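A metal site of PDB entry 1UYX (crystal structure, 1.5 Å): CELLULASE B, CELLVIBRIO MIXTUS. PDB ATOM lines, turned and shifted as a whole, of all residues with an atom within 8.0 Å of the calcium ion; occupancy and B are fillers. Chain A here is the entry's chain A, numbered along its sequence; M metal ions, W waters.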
ATOM      1  N   GLN A  14     -21.009  13.306 -18.468  1.00  0.00           N
ATOM      2  CA  GLN A  14     -19.983  12.343 -18.075  1.00  0.00           C
ATOM      3  C   GLN A  14     -18.756  12.479 -18.959  1.00  0.00           C
ATOM      4  O   GLN A  14     -18.805  13.122 -20.027  1.00  0.00           O
ATOM      5  CB  GLN A  14     -20.522  10.914 -18.156  1.00  0.00           C
ATOM      6  CG  GLN A  14     -20.723  10.380 -19.586  1.00  0.00           C
ATOM      7  CD  GLN A  14     -19.440   9.840 -20.206  1.00  0.00           C
ATOM      8  OE1 GLN A  14     -18.706   9.107 -19.558  1.00  0.00           O
ATOM      9  NE2 GLN A  14     -19.162  10.231 -21.447  1.00  0.00           N
ATOM     10  N   SER A  15     -17.678  11.857 -18.519  1.00  0.00           N
ATOM     11  CA  SER A  15     -16.458  11.740 -19.316  1.00  0.00           C
ATOM     12  C   SER A  15     -15.829  10.355 -19.162  1.00  0.00           C
ATOM     13  O   SER A  15     -15.552   9.890 -18.057  1.00  0.00           O
ATOM     14  CB  SER A  15     -15.452  12.810 -18.922  1.00  0.00           C
ATOM     15  OG  SER A  15     -14.315  12.803 -19.798  1.00  0.00           O
ATOM     16  N   GLY A  16     -15.606   9.688 -20.299  1.00  0.00           N
ATOM     17  CA  GLY A  16     -14.765   8.507 -20.359  1.00  0.00           C
ATOM     18  C   GLY A  16     -15.411   7.156 -20.104  1.00  0.00           C
ATOM     19  O   GLY A  16     -14.716   6.120 -20.156  1.00  0.00           O
ATOM     20  N   THR A  17     -16.713   7.142 -19.827  1.00  0.00           N
ATOM     21  CA  THR A  17     -17.400   5.918 -19.410  1.00  0.00           C
ATOM     22  C   THR A  17     -18.484   5.522 -20.397  1.00  0.00           C
ATOM     23  O   THR A  17     -18.755   6.233 -21.370  1.00  0.00           O
ATOM     24  CB  THR A  17     -18.042   6.073 -18.000  1.00  0.00           C
ATOM     25  OG1 THR A  17     -19.233   6.890 -18.089  1.00  0.00           O
ATOM     26  CG2 THR A  17     -17.105   6.771 -17.020  1.00  0.00           C
ATOM     27  N   GLN A  18     -19.107   4.376 -20.109  1.00  0.00           N
ATOM     28  CA  GLN A  18     -20.187   3.848 -20.928  1.00  0.00           C
ATOM     29  C   GLN A  18     -21.131   3.027 -20.061  1.00  0.00           C
ATOM     30  O   GLN A  18     -20.715   2.365 -19.127  1.00  0.00           O
ATOM     31  CB  GLN A  18     -19.570   3.002 -22.048  1.00  0.00           C
ATOM     32  CG  GLN A  18     -20.449   1.978 -22.688  1.00  0.00           C
ATOM     33  CD  GLN A  18     -19.696   1.144 -23.682  1.00  0.00           C
ATOM     34  OE1 GLN A  18     -19.070   1.677 -24.587  1.00  0.00           O
ATOM     35  NE2 GLN A  18     -19.724  -0.175 -23.503  1.00  0.00           N
ATOM     36  N   GLY A  32     -19.801   1.576 -16.563  1.00  0.00           N
ATOM     37  CA  GLY A  32     -18.584   0.797 -16.687  1.00  0.00           C
ATOM     38  C   GLY A  32     -17.505   1.539 -17.453  1.00  0.00           C
ATOM     39  O   GLY A  32     -17.651   2.709 -17.805  1.00  0.00           O
ATOM     40  N   TYR A  33     -16.415   0.832 -17.704  1.00  0.00           N
ATOM     41  CA  TYR A  33     -15.239   1.385 -18.384  1.00  0.00           C
ATOM     42  C   TYR A  33     -14.743   2.662 -17.700  1.00  0.00           C
ATOM     43  O   TYR A  33     -14.479   3.698 -18.342  1.00  0.00           O
ATOM     44  CB  TYR A  33     -15.499   1.527 -19.890  1.00  0.00           C
ATOM     45  CG  TYR A  33     -15.757   0.175 -20.498  1.00  0.00           C
ATOM     46  CD1 TYR A  33     -17.051  -0.307 -20.636  1.00  0.00           C
ATOM     47  CD2 TYR A  33     -14.708  -0.657 -20.867  1.00  0.00           C
ATOM     48  CE1 TYR A  33     -17.298  -1.571 -21.155  1.00  0.00           C
ATOM     49  CE2 TYR A  33     -14.942  -1.922 -21.390  1.00  0.00           C
ATOM     50  CZ  TYR A  33     -16.233  -2.361 -21.522  1.00  0.00           C
ATOM     51  OH  TYR A  33     -16.472  -3.619 -22.041  1.00  0.00           O
ATOM     52  N   ILE A  34     -14.613   2.541 -16.385  1.00  0.00           N
ATOM     53  CA  ILE A  34     -14.145   3.614 -15.534  1.00  0.00           C
ATOM     54  C   ILE A  34     -12.628   3.539 -15.346  1.00  0.00           C
ATOM     55  O   ILE A  34     -12.072   2.488 -15.005  1.00  0.00           O
ATOM     56  CB  ILE A  34     -14.873   3.545 -14.149  1.00  0.00           C
ATOM     57  CG1 ILE A  34     -16.394   3.594 -14.346  1.00  0.00           C
ATOM     58  CG2 ILE A  34     -14.423   4.698 -13.260  1.00  0.00           C
ATOM     59  CD1 ILE A  34     -17.207   3.510 -13.034  1.00  0.00           C
ATOM     60  N   ASP A  35     -11.973   4.673 -15.570  1.00  0.00           N
ATOM     61  CA  ASP A  35     -10.521   4.810 -15.458  1.00  0.00           C
ATOM     62  C   ASP A  35     -10.174   6.126 -14.787  1.00  0.00           C
ATOM     63  O   ASP A  35     -10.997   7.015 -14.706  1.00  0.00           O
ATOM     64  CB  ASP A  35      -9.886   4.819 -16.855  1.00  0.00           C
ATOM     65  CG  ASP A  35     -10.307   3.656 -17.688  1.00  0.00           C
ATOM     66  OD1 ASP A  35      -9.559   2.649 -17.731  1.00  0.00           O
ATOM     67  OD2 ASP A  35     -11.373   3.707 -18.353  1.00  0.00           O
ATOM     68  N   ALA A  36      -8.920   6.264 -14.347  1.00  0.00           N
ATOM     69  CA  ALA A  36      -8.435   7.519 -13.781  1.00  0.00           C
ATOM     70  C   ALA A  36      -8.728   8.706 -14.698  1.00  0.00           C
ATOM     71  O   ALA A  36      -8.406   8.678 -15.888  1.00  0.00           O
ATOM     72  CB  ALA A  36      -6.948   7.426 -13.515  1.00  0.00           C
ATOM     73  N   GLY A  37      -9.337   9.741 -14.124  1.00  0.00           N
ATOM     74  CA  GLY A  37      -9.701  10.945 -14.839  1.00  0.00           C
ATOM     75  C   GLY A  37     -11.166  11.011 -15.243  1.00  0.00           C
ATOM     76  O   GLY A  37     -11.703  12.104 -15.461  1.00  0.00           O
ATOM     77  N   ASP A  38     -11.805   9.846 -15.346  1.00  0.00           N
ATOM     78  CA  ASP A  38     -13.209   9.776 -15.754  1.00  0.00           C
ATOM     79  C   ASP A  38     -14.098  10.355 -14.663  1.00  0.00           C
ATOM     80  O   ASP A  38     -13.716  10.385 -13.494  1.00  0.00           O
ATOM     81  CB  ASP A  38     -13.616   8.329 -15.997  1.00  0.00           C
ATOM     82  CG  ASP A  38     -12.977   7.707 -17.253  1.00  0.00           C
ATOM     83  OD1 ASP A  38     -12.325   8.433 -18.052  1.00  0.00           O
ATOM     84  OD2 ASP A  38     -13.102   6.475 -17.535  1.00  0.00           O
ATOM     85  N   TRP A  39     -15.262  10.826 -15.055  1.00  0.00           N
ATOM     86  CA  TRP A  39     -16.171  11.460 -14.103  1.00  0.00           C
ATOM     87  C   TRP A  39     -17.622  11.386 -14.524  1.00  0.00           C
ATOM     88  O   TRP A  39     -17.960  11.113 -15.669  1.00  0.00           O
ATOM     89  CB  TRP A  39     -15.751  12.902 -13.810  1.00  0.00           C
ATOM     90  CG  TRP A  39     -15.625  13.831 -14.993  1.00  0.00           C
ATOM     91  CD1 TRP A  39     -14.464  14.193 -15.625  1.00  0.00           C
ATOM     92  CD2 TRP A  39     -16.681  14.559 -15.640  1.00  0.00           C
ATOM     93  NE1 TRP A  39     -14.745  15.092 -16.629  1.00  0.00           N
ATOM     94  CE2 TRP A  39     -16.088  15.333 -16.671  1.00  0.00           C
ATOM     95  CE3 TRP A  39     -18.066  14.625 -15.465  1.00  0.00           C
ATOM     96  CZ2 TRP A  39     -16.840  16.155 -17.511  1.00  0.00           C
ATOM     97  CZ3 TRP A  39     -18.798  15.453 -16.308  1.00  0.00           C
ATOM     98  CH2 TRP A  39     -18.186  16.203 -17.320  1.00  0.00           C
ATOM     99  N   ALA A 115     -13.312   9.550 -10.777  1.00  0.00           N
ATOM    100  CA  ALA A 115     -12.525   8.344 -10.567  1.00  0.00           C
ATOM    101  C   ALA A 115     -11.041   8.680 -10.470  1.00  0.00           C
ATOM    102  O   ALA A 115     -10.461   9.238 -11.386  1.00  0.00           O
ATOM    103  CB  ALA A 115     -12.756   7.360 -11.697  1.00  0.00           C
ATOM    104  N   GLY A 118      -9.230   3.418 -11.781  1.00  0.00           N
ATOM    105  CA  GLY A 118     -10.277   2.587 -12.333  1.00  0.00           C
ATOM    106  C   GLY A 118     -10.336   1.185 -11.759  1.00  0.00           C
ATOM    107  O   GLY A 118      -9.810   0.926 -10.677  1.00  0.00           O
HETATM  108 CA    CA M   1     -12.939   5.020 -19.310  1.00  0.00          CA
HETATM  109  O   HOH W   1     -11.458   6.696 -19.986  1.00  0.00           O
HETATM  110  O   HOH W   2     -12.308   3.733 -21.023  1.00  0.00           O
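The backbone carbonyl oxygen of Asp 38 lies within hydrogen-bond range of the backbone NH of Ala 115 (2.9 Å). The backbone NH of Gly 16 lies within hydrogen-bond range of the side-chain amide oxygen of Gln 14, 3.2 Å away.
Water W2 is bound to the calcium ion, 2.2 Å away. O of Tyr 33 is bound to the calcium ion. O of Gly 16 is bound to the calcium ion. OD2 of Asp 35 binds the calcium ion (2.3 Å). OD2 of Asp 38 binds the calcium ion (2.3 Å). Water W1 binds the calcium ion (2.3 Å).
Within 4 Å of the calcium ion: Gly 16, Tyr 33, Asp 35 and Asp 38.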
